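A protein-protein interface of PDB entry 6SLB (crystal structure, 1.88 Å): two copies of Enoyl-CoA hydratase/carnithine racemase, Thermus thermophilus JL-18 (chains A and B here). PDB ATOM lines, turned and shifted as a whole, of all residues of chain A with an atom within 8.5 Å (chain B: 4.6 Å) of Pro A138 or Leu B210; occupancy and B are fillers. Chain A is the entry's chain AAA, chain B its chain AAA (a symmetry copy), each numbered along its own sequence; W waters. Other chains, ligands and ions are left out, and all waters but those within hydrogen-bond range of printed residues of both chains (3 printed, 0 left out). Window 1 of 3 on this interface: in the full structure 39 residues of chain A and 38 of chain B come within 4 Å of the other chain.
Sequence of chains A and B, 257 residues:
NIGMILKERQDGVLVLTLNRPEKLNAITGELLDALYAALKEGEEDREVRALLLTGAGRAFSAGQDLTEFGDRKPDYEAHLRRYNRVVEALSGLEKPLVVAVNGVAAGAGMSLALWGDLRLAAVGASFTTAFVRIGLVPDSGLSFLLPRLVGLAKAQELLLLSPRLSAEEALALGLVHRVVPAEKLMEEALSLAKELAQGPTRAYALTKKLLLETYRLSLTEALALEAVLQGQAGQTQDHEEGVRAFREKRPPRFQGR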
ATOM      1  N   LEU A  80      -4.024 -25.857   6.143  1.00  0.00           N
ATOM      2  CA  LEU A  80      -2.548 -25.812   6.020  1.00  0.00           C
ATOM      3  C   LEU A  80      -1.917 -27.011   6.738  1.00  0.00           C
ATOM      4  O   LEU A  80      -0.894 -27.485   6.243  1.00  0.00           O
ATOM      5  CB  LEU A  80      -2.012 -24.458   6.497  1.00  0.00           C
ATOM      6  CG  LEU A  80      -1.916 -23.411   5.386  1.00  0.00           C
ATOM      7  CD1 LEU A  80      -1.212 -22.150   5.893  1.00  0.00           C
ATOM      8  CD2 LEU A  80      -1.191 -23.973   4.168  1.00  0.00           C
ATOM      9  N   GLY A 107       3.294 -18.678  -5.776  1.00  0.00           N
ATOM     10  CA  GLY A 107       2.651 -19.032  -4.495  1.00  0.00           C
ATOM     11  C   GLY A 107       3.238 -20.298  -3.903  1.00  0.00           C
ATOM     12  O   GLY A 107       4.473 -20.423  -3.826  1.00  0.00           O
ATOM     13  N   ALA A 108       2.393 -21.246  -3.488  1.00  0.00           N
ATOM     14  CA  ALA A 108       2.865 -22.541  -2.962  1.00  0.00           C
ATOM     15  C   ALA A 108       3.658 -23.308  -4.020  1.00  0.00           C
ATOM     16  O   ALA A 108       4.426 -24.182  -3.619  1.00  0.00           O
ATOM     17  CB  ALA A 108       1.703 -23.348  -2.403  1.00  0.00           C
ATOM     18  N   SER A 111       6.977 -22.075  -3.276  1.00  0.00           N
ATOM     19  CA  SER A 111       7.358 -22.739  -2.001  1.00  0.00           C
ATOM     20  C   SER A 111       7.921 -24.137  -2.311  1.00  0.00           C
ATOM     21  O   SER A 111       9.016 -24.460  -1.842  1.00  0.00           O
ATOM     22  CB  SER A 111       6.220 -22.851  -1.007  1.00  0.00           C
ATOM     23  OG  SER A 111       5.597 -21.599  -0.724  1.00  0.00           O
ATOM     24  N   THR A 129       5.976 -14.688  -5.874  1.00  0.00           N
ATOM     25  CA  THR A 129       5.482 -15.089  -4.536  1.00  0.00           C
ATOM     26  C   THR A 129       3.952 -15.209  -4.587  1.00  0.00           C
ATOM     27  O   THR A 129       3.457 -16.149  -3.989  1.00  0.00           O
ATOM     28  CB  THR A 129       6.028 -14.170  -3.443  1.00  0.00           C
ATOM     29  OG1 THR A 129       5.587 -12.840  -3.687  1.00  0.00           O
ATOM     30  CG2 THR A 129       7.541 -14.220  -3.361  1.00  0.00           C
ATOM     31  N   ALA A 130       3.245 -14.251  -5.181  1.00  0.00           N
ATOM     32  CA  ALA A 130       1.798 -14.357  -5.523  1.00  0.00           C
ATOM     33  C   ALA A 130       0.857 -14.135  -4.328  1.00  0.00           C
ATOM     34  O   ALA A 130      -0.180 -13.470  -4.540  1.00  0.00           O
ATOM     35  CB  ALA A 130       1.496 -15.682  -6.183  1.00  0.00           C
ATOM     36  N   PHE A 131       1.167 -14.659  -3.132  1.00  0.00           N
ATOM     37  CA  PHE A 131       0.215 -14.677  -1.986  1.00  0.00           C
ATOM     38  C   PHE A 131      -0.376 -13.279  -1.736  1.00  0.00           C
ATOM     39  O   PHE A 131      -1.600 -13.126  -1.551  1.00  0.00           O
ATOM     40  CB  PHE A 131       0.902 -15.160  -0.712  1.00  0.00           C
ATOM     41  CG  PHE A 131       1.360 -16.591  -0.752  1.00  0.00           C
ATOM     42  CD1 PHE A 131       0.477 -17.620  -0.516  1.00  0.00           C
ATOM     43  CD2 PHE A 131       2.680 -16.894  -1.000  1.00  0.00           C
ATOM     44  CE1 PHE A 131       0.915 -18.926  -0.497  1.00  0.00           C
ATOM     45  CE2 PHE A 131       3.107 -18.215  -1.021  1.00  0.00           C
ATOM     46  CZ  PHE A 131       2.230 -19.220  -0.770  1.00  0.00           C
ATOM     47  N   VAL A 132       0.472 -12.248  -1.736  1.00  0.00           N
ATOM     48  CA  VAL A 132       0.029 -10.887  -1.337  1.00  0.00           C
ATOM     49  C   VAL A 132      -1.015 -10.375  -2.334  1.00  0.00           C
ATOM     50  O   VAL A 132      -1.920  -9.638  -1.901  1.00  0.00           O
ATOM     51  CB  VAL A 132       1.214  -9.917  -1.152  1.00  0.00           C
ATOM     52  CG1 VAL A 132       1.837  -9.505  -2.471  1.00  0.00           C
ATOM     53  CG2 VAL A 132       0.770  -8.711  -0.355  1.00  0.00           C
ATOM     54  N   GLY A 135      -4.260 -11.283  -1.065  1.00  0.00           N
ATOM     55  CA  GLY A 135      -4.457 -10.809   0.326  1.00  0.00           C
ATOM     56  C   GLY A 135      -4.062 -11.843   1.354  1.00  0.00           C
ATOM     57  O   GLY A 135      -4.598 -11.782   2.450  1.00  0.00           O
ATOM     58  N   LEU A 136      -3.117 -12.737   1.031  1.00  0.00           N
ATOM     59  CA  LEU A 136      -2.647 -13.827   1.913  1.00  0.00           C
ATOM     60  C   LEU A 136      -1.165 -13.625   2.236  1.00  0.00           C
ATOM     61  O   LEU A 136      -0.496 -12.793   1.587  1.00  0.00           O
ATOM     62  CB  LEU A 136      -2.836 -15.171   1.221  1.00  0.00           C
ATOM     63  CG  LEU A 136      -4.283 -15.593   1.039  1.00  0.00           C
ATOM     64  CD1 LEU A 136      -4.333 -16.962   0.418  1.00  0.00           C
ATOM     65  CD2 LEU A 136      -5.032 -15.557   2.370  1.00  0.00           C
ATOM     66  N   VAL A 137      -0.686 -14.405   3.193  1.00  0.00           N
ATOM     67  CA  VAL A 137       0.730 -14.371   3.657  1.00  0.00           C
ATOM     68  C   VAL A 137       1.425 -15.548   2.990  1.00  0.00           C
ATOM     69  O   VAL A 137       0.776 -16.474   2.517  1.00  0.00           O
ATOM     70  CB  VAL A 137       0.825 -14.462   5.195  1.00  0.00           C
ATOM     71  CG1 VAL A 137      -0.025 -13.395   5.883  1.00  0.00           C
ATOM     72  CG2 VAL A 137       0.475 -15.837   5.705  1.00  0.00           C
ATOM     73  N   PRO A 138       2.769 -15.551   2.922  1.00  0.00           N
ATOM     74  CA  PRO A 138       3.488 -16.688   2.348  1.00  0.00           C
ATOM     75  C   PRO A 138       3.292 -17.910   3.255  1.00  0.00           C
ATOM     76  O   PRO A 138       3.268 -17.781   4.492  1.00  0.00           O
ATOM     77  CB  PRO A 138       4.934 -16.187   2.315  1.00  0.00           C
ATOM     78  CG  PRO A 138       4.998 -15.162   3.446  1.00  0.00           C
ATOM     79  CD  PRO A 138       3.655 -14.465   3.379  1.00  0.00           C
ATOM     80  N   ASP A 139       3.068 -19.063   2.648  1.00  0.00           N
ATOM     81  CA  ASP A 139       2.830 -20.316   3.395  1.00  0.00           C
ATOM     82  C   ASP A 139       3.630 -21.430   2.741  1.00  0.00           C
ATOM     83  O   ASP A 139       4.517 -21.128   1.874  1.00  0.00           O
ATOM     84  CB  ASP A 139       1.326 -20.586   3.532  1.00  0.00           C
ATOM     85  CG  ASP A 139       0.576 -21.086   2.303  1.00  0.00           C
ATOM     86  OD1 ASP A 139       1.186 -21.722   1.393  1.00  0.00           O
ATOM     87  OD2 ASP A 139      -0.660 -20.910   2.308  1.00  0.00           O
ATOM     88  N   SER A 140       3.394 -22.660   3.202  1.00  0.00           N
ATOM     89  CA  SER A 140       4.114 -23.856   2.720  1.00  0.00           C
ATOM     90  C   SER A 140       5.619 -23.657   2.879  1.00  0.00           C
ATOM     91  O   SER A 140       6.405 -24.271   2.111  1.00  0.00           O
ATOM     92  CB  SER A 140       3.710 -24.157   1.309  1.00  0.00           C
ATOM     93  OG  SER A 140       2.303 -24.036   1.188  1.00  0.00           O
ATOM     94  N   GLY A 141       6.001 -22.990   3.964  1.00  0.00           N
ATOM     95  CA  GLY A 141       7.406 -22.805   4.358  1.00  0.00           C
ATOM     96  C   GLY A 141       8.076 -21.685   3.589  1.00  0.00           C
ATOM     97  O   GLY A 141       9.294 -21.563   3.723  1.00  0.00           O
ATOM     98  N   LEU A 142       7.339 -20.891   2.796  1.00  0.00           N
ATOM     99  CA  LEU A 142       8.004 -19.805   2.021  1.00  0.00           C
ATOM    100  C   LEU A 142       8.550 -18.725   2.964  1.00  0.00           C
ATOM    101  O   LEU A 142       9.605 -18.134   2.617  1.00  0.00           O
ATOM    102  CB  LEU A 142       7.058 -19.238   0.956  1.00  0.00           C
ATOM    103  CG  LEU A 142       7.686 -18.229  -0.006  1.00  0.00           C
ATOM    104  CD1 LEU A 142       8.883 -18.808  -0.717  1.00  0.00           C
ATOM    105  CD2 LEU A 142       6.677 -17.750  -1.028  1.00  0.00           C
ATOM    106  N   SER A 143       7.862 -18.407   4.073  1.00  0.00           N
ATOM    107  CA  SER A 143       8.334 -17.378   5.043  1.00  0.00           C
ATOM    108  C   SER A 143       9.589 -17.880   5.766  1.00  0.00           C
ATOM    109  O   SER A 143      10.361 -17.026   6.198  1.00  0.00           O
ATOM    110  CB  SER A 143       7.291 -16.946   6.058  1.00  0.00           C
ATOM    111  OG  SER A 143       7.081 -17.958   7.030  1.00  0.00           O
ATOM    112  N   PHE A 144       9.786 -19.203   5.868  1.00  0.00           N
ATOM    113  CA  PHE A 144      11.014 -19.839   6.413  1.00  0.00           C
ATOM    114  C   PHE A 144      12.147 -19.814   5.350  1.00  0.00           C
ATOM    115  O   PHE A 144      13.265 -19.314   5.615  1.00  0.00           O
ATOM    116  CB  PHE A 144      10.651 -21.260   6.869  1.00  0.00           C
ATOM    117  CG  PHE A 144      11.780 -22.067   7.450  1.00  0.00           C
ATOM    118  CD1 PHE A 144      12.601 -22.830   6.637  1.00  0.00           C
ATOM    119  CD2 PHE A 144      11.987 -22.096   8.814  1.00  0.00           C
ATOM    120  CE1 PHE A 144      13.620 -23.602   7.180  1.00  0.00           C
ATOM    121  CE2 PHE A 144      13.011 -22.846   9.355  1.00  0.00           C
ATOM    122  CZ  PHE A 144      13.834 -23.586   8.537  1.00  0.00           C
ATOM    123  N   LEU A 145      11.884 -20.354   4.157  1.00  0.00           N
ATOM    124  CA  LEU A 145      12.944 -20.587   3.135  1.00  0.00           C
ATOM    125  C   LEU A 145      13.435 -19.262   2.546  1.00  0.00           C
ATOM    126  O   LEU A 145      14.656 -19.117   2.378  1.00  0.00           O
ATOM    127  CB  LEU A 145      12.432 -21.488   2.012  1.00  0.00           C
ATOM    128  CG  LEU A 145      12.518 -22.996   2.255  1.00  0.00           C
ATOM    129  CD1 LEU A 145      11.942 -23.760   1.070  1.00  0.00           C
ATOM    130  CD2 LEU A 145      13.949 -23.432   2.533  1.00  0.00           C
ATOM    131  N   LEU A 146      12.526 -18.365   2.144  1.00  0.00           N
ATOM    132  CA  LEU A 146      12.908 -17.234   1.269  1.00  0.00           C
ATOM    133  C   LEU A 146      13.979 -16.333   1.905  1.00  0.00           C
ATOM    134  O   LEU A 146      15.001 -16.066   1.260  1.00  0.00           O
ATOM    135  CB  LEU A 146      11.671 -16.460   0.800  1.00  0.00           C
ATOM    136  CG  LEU A 146      11.959 -15.483  -0.345  1.00  0.00           C
ATOM    137  CD1 LEU A 146      12.531 -16.189  -1.577  1.00  0.00           C
ATOM    138  CD2 LEU A 146      10.703 -14.704  -0.729  1.00  0.00           C
ATOM    139  N   PRO A 147      13.846 -15.834   3.160  1.00  0.00           N
ATOM    140  CA  PRO A 147      14.884 -14.985   3.748  1.00  0.00           C
ATOM    141  C   PRO A 147      16.222 -15.739   3.922  1.00  0.00           C
ATOM    142  O   PRO A 147      17.265 -15.168   3.701  1.00  0.00           O
ATOM    143  CB  PRO A 147      14.317 -14.600   5.122  1.00  0.00           C
ATOM    144  CG  PRO A 147      12.842 -14.827   4.986  1.00  0.00           C
ATOM    145  CD  PRO A 147      12.691 -15.998   4.061  1.00  0.00           C
ATOM    146  N   ARG A 148      16.167 -17.032   4.223  1.00  0.00           N
ATOM    147  CA  ARG A 148      17.385 -17.886   4.339  1.00  0.00           C
ATOM    148  C   ARG A 148      18.070 -17.958   2.966  1.00  0.00           C
ATOM    149  O   ARG A 148      19.327 -17.829   2.892  1.00  0.00           O
ATOM    150  CB  ARG A 148      16.985 -19.268   4.881  1.00  0.00           C
ATOM    151  CG  ARG A 148      16.559 -19.280   6.341  1.00  0.00           C
ATOM    152  CD  ARG A 148      15.933 -20.605   6.734  1.00  0.00           C
ATOM    153  NE  ARG A 148      15.757 -20.770   8.165  1.00  0.00           N
ATOM    154  CZ  ARG A 148      14.863 -20.146   8.915  1.00  0.00           C
ATOM    155  NH1 ARG A 148      13.968 -19.322   8.380  1.00  0.00           N
ATOM    156  NH2 ARG A 148      14.827 -20.397  10.217  1.00  0.00           N
ATOM    157  N   LEU A 152      17.118 -11.199   3.895  1.00  0.00           N
ATOM    158  CA  LEU A 152      15.860 -10.511   4.279  1.00  0.00           C
ATOM    159  C   LEU A 152      15.531  -9.371   3.312  1.00  0.00           C
ATOM    160  O   LEU A 152      14.368  -9.146   3.052  1.00  0.00           O
ATOM    161  CB  LEU A 152      15.982  -9.989   5.716  1.00  0.00           C
ATOM    162  CG  LEU A 152      14.808  -9.126   6.168  1.00  0.00           C
ATOM    163  CD1 LEU A 152      13.538  -9.968   6.134  1.00  0.00           C
ATOM    164  CD2 LEU A 152      15.060  -8.566   7.565  1.00  0.00           C
ATOM    165  N   ALA A 155      13.846 -10.829   0.269  1.00  0.00           N
ATOM    166  CA  ALA A 155      12.604 -11.516   0.702  1.00  0.00           C
ATOM    167  C   ALA A 155      11.496 -10.474   0.914  1.00  0.00           C
ATOM    168  O   ALA A 155      10.384 -10.653   0.389  1.00  0.00           O
ATOM    169  CB  ALA A 155      12.852 -12.319   1.939  1.00  0.00           C
ATOM    170  N   LEU A 158      10.382  -9.204  -2.608  1.00  0.00           N
ATOM    171  CA  LEU A 158       9.712 -10.287  -3.375  1.00  0.00           C
ATOM    172  C   LEU A 158       8.308 -10.569  -2.795  1.00  0.00           C
ATOM    173  O   LEU A 158       7.384 -10.830  -3.582  1.00  0.00           O
ATOM    174  CB  LEU A 158      10.580 -11.535  -3.369  1.00  0.00           C
ATOM    175  CG  LEU A 158      11.872 -11.459  -4.182  1.00  0.00           C
ATOM    176  CD1 LEU A 158      12.542 -12.819  -4.213  1.00  0.00           C
ATOM    177  CD2 LEU A 158      11.624 -10.947  -5.571  1.00  0.00           C
ATOM    178  N   LEU A 159       8.152 -10.530  -1.482  1.00  0.00           N
ATOM    179  CA  LEU A 159       6.914 -10.941  -0.807  1.00  0.00           C
ATOM    180  C   LEU A 159       5.914  -9.784  -0.828  1.00  0.00           C
ATOM    181  O   LEU A 159       4.718 -10.059  -1.120  1.00  0.00           O
ATOM    182  CB  LEU A 159       7.253 -11.384   0.610  1.00  0.00           C
ATOM    183  CG  LEU A 159       7.921 -12.749   0.718  1.00  0.00           C
ATOM    184  CD1 LEU A 159       8.370 -12.992   2.130  1.00  0.00           C
ATOM    185  CD2 LEU A 159       6.935 -13.837   0.273  1.00  0.00           C
ATOM    186  N   LEU A 160       6.356  -8.558  -0.509  1.00  0.00           N
ATOM    187  CA  LEU A 160       5.460  -7.381  -0.387  1.00  0.00           C
ATOM    188  C   LEU A 160       4.971  -6.889  -1.752  1.00  0.00           C
ATOM    189  O   LEU A 160       3.775  -6.468  -1.840  1.00  0.00           O
ATOM    190  CB  LEU A 160       6.169  -6.270   0.406  1.00  0.00           C
ATOM    191  CG  LEU A 160       6.512  -6.660   1.842  1.00  0.00           C
ATOM    192  CD1 LEU A 160       7.253  -5.541   2.559  1.00  0.00           C
ATOM    193  CD2 LEU A 160       5.268  -7.103   2.632  1.00  0.00           C
ATOM    194  N   LEU B 206       0.804  -9.058   8.600  1.00  0.00           N
ATOM    195  CA  LEU B 206       1.042 -10.457   9.019  1.00  0.00           C
ATOM    196  C   LEU B 206       2.304 -11.006   8.336  1.00  0.00           C
ATOM    197  O   LEU B 206       3.030 -11.780   8.985  1.00  0.00           O
ATOM    198  CB  LEU B 206      -0.197 -11.294   8.673  1.00  0.00           C
ATOM    199  CG  LEU B 206      -1.480 -10.832   9.379  1.00  0.00           C
ATOM    200  CD1 LEU B 206      -2.701 -11.589   8.879  1.00  0.00           C
ATOM    201  CD2 LEU B 206      -1.344 -10.993  10.880  1.00  0.00           C
ATOM    202  N   THR B 207       2.554 -10.623   7.091  1.00  0.00           N
ATOM    203  CA  THR B 207       3.791 -11.011   6.373  1.00  0.00           C
ATOM    204  C   THR B 207       4.997 -10.458   7.150  1.00  0.00           C
ATOM    205  O   THR B 207       5.985 -11.185   7.344  1.00  0.00           O
ATOM    206  CB  THR B 207       3.757 -10.548   4.915  1.00  0.00           C
ATOM    207  OG1 THR B 207       2.689 -11.190   4.202  1.00  0.00           O
ATOM    208  CG2 THR B 207       5.071 -10.831   4.224  1.00  0.00           C
ATOM    209  N   LYS B 208       4.919  -9.211   7.613  1.00  0.00           N
ATOM    210  CA  LYS B 208       5.995  -8.585   8.420  1.00  0.00           C
ATOM    211  C   LYS B 208       6.223  -9.388   9.713  1.00  0.00           C
ATOM    212  O   LYS B 208       7.394  -9.566  10.077  1.00  0.00           O
ATOM    213  CB  LYS B 208       5.664  -7.126   8.720  1.00  0.00           C
ATOM    214  CG  LYS B 208       5.827  -6.188   7.540  1.00  0.00           C
ATOM    215  CD  LYS B 208       5.320  -4.789   7.801  1.00  0.00           C
ATOM    216  CE  LYS B 208       5.937  -4.080   8.994  1.00  0.00           C
ATOM    217  NZ  LYS B 208       5.838  -2.606   8.813  1.00  0.00           N
ATOM    218  N   LYS B 209       5.165  -9.887  10.352  1.00  0.00           N
ATOM    219  CA  LYS B 209       5.295 -10.681  11.603  1.00  0.00           C
ATOM    220  C   LYS B 209       6.046 -11.982  11.294  1.00  0.00           C
ATOM    221  O   LYS B 209       6.909 -12.347  12.058  1.00  0.00           O
ATOM    222  CB  LYS B 209       3.935 -10.999  12.229  1.00  0.00           C
ATOM    223  CG  LYS B 209       3.048  -9.812  12.541  1.00  0.00           C
ATOM    224  CD  LYS B 209       1.918 -10.147  13.514  1.00  0.00           C
ATOM    225  CE  LYS B 209       0.953  -8.990  13.729  1.00  0.00           C
ATOM    226  NZ  LYS B 209       1.648  -7.683  13.876  1.00  0.00           N
ATOM    227  N   LEU B 210       5.722 -12.672  10.191  1.00  0.00           N
ATOM    228  CA  LEU B 210       6.429 -13.916   9.807  1.00  0.00           C
ATOM    229  C   LEU B 210       7.916 -13.645   9.590  1.00  0.00           C
ATOM    230  O   LEU B 210       8.725 -14.435  10.113  1.00  0.00           O
ATOM    231  CB  LEU B 210       5.815 -14.475   8.530  1.00  0.00           C
ATOM    232  CG  LEU B 210       4.454 -15.126   8.741  1.00  0.00           C
ATOM    233  CD1 LEU B 210       3.792 -15.402   7.407  1.00  0.00           C
ATOM    234  CD2 LEU B 210       4.598 -16.399   9.566  1.00  0.00           C
ATOM    235  N   LEU B 211       8.241 -12.581   8.846  1.00  0.00           N
ATOM    236  CA  LEU B 211       9.647 -12.201   8.527  1.00  0.00           C
ATOM    237  C   LEU B 211      10.422 -11.894   9.802  1.00  0.00           C
ATOM    238  O   LEU B 211      11.575 -12.317   9.877  1.00  0.00           O
ATOM    239  CB  LEU B 211       9.684 -11.010   7.571  1.00  0.00           C
ATOM    240  CG  LEU B 211       9.251 -11.369   6.160  1.00  0.00           C
ATOM    241  CD1 LEU B 211       9.271 -10.186   5.240  1.00  0.00           C
ATOM    242  CD2 LEU B 211      10.098 -12.497   5.632  1.00  0.00           C
ATOM    243  N   LEU B 212       9.819 -11.168  10.749  1.00  0.00           N
ATOM    244  CA  LEU B 212      10.483 -10.820  12.046  1.00  0.00           C
ATOM    245  C   LEU B 212      10.875 -12.077  12.836  1.00  0.00           C
ATOM    246  O   LEU B 212      11.946 -12.086  13.500  1.00  0.00           O
ATOM    247  CB  LEU B 212       9.524  -9.929  12.852  1.00  0.00           C
ATOM    248  CG  LEU B 212      10.199  -9.176  13.986  1.00  0.00           C
ATOM    249  CD1 LEU B 212      11.252  -8.228  13.406  1.00  0.00           C
ATOM    250  CD2 LEU B 212       9.163  -8.429  14.831  1.00  0.00           C
ATOM    251  N   GLU B 213      10.038 -13.115  12.807  1.00  0.00           N
ATOM    252  CA  GLU B 213      10.195 -14.346  13.638  1.00  0.00           C
ATOM    253  C   GLU B 213      10.966 -15.462  12.915  1.00  0.00           C
ATOM    254  O   GLU B 213      11.437 -16.349  13.596  1.00  0.00           O
ATOM    255  CB  GLU B 213       8.806 -14.861  14.006  1.00  0.00           C
ATOM    256  CG  GLU B 213       7.963 -13.790  14.670  1.00  0.00           C
ATOM    257  CD  GLU B 213       6.884 -14.310  15.597  1.00  0.00           C
ATOM    258  OE1 GLU B 213       7.188 -15.240  16.364  1.00  0.00           O
ATOM    259  OE2 GLU B 213       5.749 -13.768  15.560  1.00  0.00           O
ATOM    260  N   THR B 214      11.108 -15.411  11.599  1.00  0.00           N
ATOM    261  CA  THR B 214      11.529 -16.557  10.748  1.00  0.00           C
ATOM    262  C   THR B 214      12.827 -17.218  11.250  1.00  0.00           C
ATOM    263  O   THR B 214      12.831 -18.441  11.368  1.00  0.00           O
ATOM    264  CB  THR B 214      11.629 -16.136   9.279  1.00  0.00           C
ATOM    265  OG1 THR B 214      11.592 -17.340   8.506  1.00  0.00           O
ATOM    266  CG2 THR B 214      12.867 -15.334   8.965  1.00  0.00           C
ATOM    267  N   LEU B 225       2.995 -21.158  12.674  1.00  0.00           N
ATOM    268  CA  LEU B 225       2.669 -19.718  12.686  1.00  0.00           C
ATOM    269  C   LEU B 225       2.075 -19.306  11.331  1.00  0.00           C
ATOM    270  O   LEU B 225       1.143 -18.447  11.306  1.00  0.00           O
ATOM    271  CB  LEU B 225       3.925 -18.915  13.032  1.00  0.00           C
ATOM    272  CG  LEU B 225       3.738 -17.415  13.183  1.00  0.00           C
ATOM    273  CD1 LEU B 225       2.779 -17.072  14.308  1.00  0.00           C
ATOM    274  CD2 LEU B 225       5.106 -16.750  13.404  1.00  0.00           C
ATOM    275  N   GLU B 226       2.603 -19.850  10.240  1.00  0.00           N
ATOM    276  CA  GLU B 226       2.057 -19.601   8.885  1.00  0.00           C
ATOM    277  C   GLU B 226       0.565 -19.988   8.900  1.00  0.00           C
ATOM    278  O   GLU B 226      -0.265 -19.223   8.415  1.00  0.00           O
ATOM    279  CB  GLU B 226       2.850 -20.415   7.847  1.00  0.00           C
ATOM    280  CG  GLU B 226       4.135 -19.749   7.344  1.00  0.00           C
ATOM    281  CD  GLU B 226       4.986 -20.628   6.422  1.00  0.00           C
ATOM    282  OE1 GLU B 226       4.532 -21.741   6.073  1.00  0.00           O
ATOM    283  OE2 GLU B 226       6.100 -20.195   6.025  1.00  0.00           O
ATOM    284  N   LEU B 229      -1.509 -17.410  11.020  1.00  0.00           N
ATOM    285  CA  LEU B 229      -1.622 -16.066  10.392  1.00  0.00           C
ATOM    286  C   LEU B 229      -2.379 -16.161   9.061  1.00  0.00           C
ATOM    287  O   LEU B 229      -3.101 -15.206   8.735  1.00  0.00           O
ATOM    288  CB  LEU B 229      -0.227 -15.444  10.257  1.00  0.00           C
ATOM    289  CG  LEU B 229       0.480 -15.181  11.578  1.00  0.00           C
ATOM    290  CD1 LEU B 229       1.733 -14.316  11.359  1.00  0.00           C
ATOM    291  CD2 LEU B 229      -0.460 -14.521  12.598  1.00  0.00           C
HETATM  292  O   HOH W   1       2.132 -11.843   1.507  1.00  0.00           O
HETATM  293  O   HOH W   2       2.353 -23.373   5.828  1.00  0.00           O
HETATM  294  O   HOH W   3       8.557 -18.252   9.126  1.00  0.00           O
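Pro A138 touches three residues of chain B.
Of the printed residues of chain B, Arg A148 touches Thr B214 (3.0 Å).
Of the printed residues of chain B, Ser A143 touches Leu B210 (3.8 Å), Thr B214 (2.6 Å) and Glu B226 (2.6 Å).
The nearest printed residue of chain B that does not touch Pro A138 is Leu B211 (6.2 Å).
The nearest residue of chain A that does not touch Leu B210 is Asp A139 (6.0 Å).
The nearest printed residue of chain B that does not touch Ser A140 is Leu B210 (8.4 Å).
Among the printed residues, pairs that only touch across the chains: Leu A80 with Glu B226 (3.98 Å), Val A137 with Leu B206 (3.5 Å), Val A137 with Thr B207 (3.8 Å), Val A137 with Leu B210 (3.8 Å), Pro A138 with Thr B207 (3.5 Å), Pro A138 with Leu B210 (3.8 Å), Pro A138 with Glu B226 (3.6 Å), Asp A139 with Glu B226 (3.5 Å), Leu A142 with Glu B226 (3.5 Å), Ser A143 with Leu B210 (3.8 Å), Phe A144 with Thr B214 (3.3 Å), Phe A144 with Glu B226 (3.8 Å), Pro A147 with Leu B211 (3.7 Å) and Leu A159 with Leu B211 (3.9 Å).
The side-chain carboxylate of Glu B226 sits at hydrogen-bond distance from the backbone NH of Ser A140, 3.2 Å away.
OE1 of Glu B226 lies within hydrogen-bond range of N of Gly A141, at 2.9 Å.
The backbone carbonyl oxygen of Ser A143 lies within hydrogen-bond range of the side-chain hydroxyl of Thr B214 (2.6 Å).
The side-chain hydroxyl (OG) of Ser A143 sits at hydrogen-bond distance from the side-chain carboxylate (OE2) of Glu B226, at 2.6 Å.
The guanidinium group (NH2) of Arg A148 lies within hydrogen-bond range of the backbone carbonyl oxygen (O) of Thr B214 (3.0 Å).
Water W3 lies within hydrogen-bond range of the side-chain hydroxyl (OG) of Ser A143 and the side-chain hydroxyl (OG1) of Thr B214.
Water W2 bridges the side-chain carboxylate (OE1) of Glu B226 (2.7 Å) and the backbone NH (N) of Ser A140 (2.9 Å).
Water W1 bridges the backbone carbonyl oxygen of Leu A136 (2.8 Å) and the side-chain hydroxyl of Thr B207 (2.8 Å).
The backbone carbonyl oxygen (O) of Asp A139 lies within hydrogen-bond range of the side-chain hydroxyl (OG) of Ser A111 (2.9 Å).
OD1 of Asp A139 lies within hydrogen-bond range of OG of Ser A140.
NH1 of Arg A148 lies within hydrogen-bond range of O of Phe A144 (2.9 Å).
No position is printed for both chains.
Of the 12 printed residues of chain B, 6 touch a printed residue of chain A.
Printed residues of chain B that touch a printed residue of chain A: Leu B206, Thr B207, Leu B210, Leu B211, Thr B214 and Glu B226.
Hydrophobic or aromatic side chains of chain B that line the printed part of chain A: Leu B206, Leu B210 and Leu B211.
Hydrophobic or aromatic side chains of chain A within 4 Å of the printed part of chain B: Leu A80, Val A137, Pro A138, Pro A147 and Leu A159.
Among the printed residues, no Asp or Glu carboxylate lies within 4 Å of a Lys or Arg side-chain nitrogen of the other chain.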
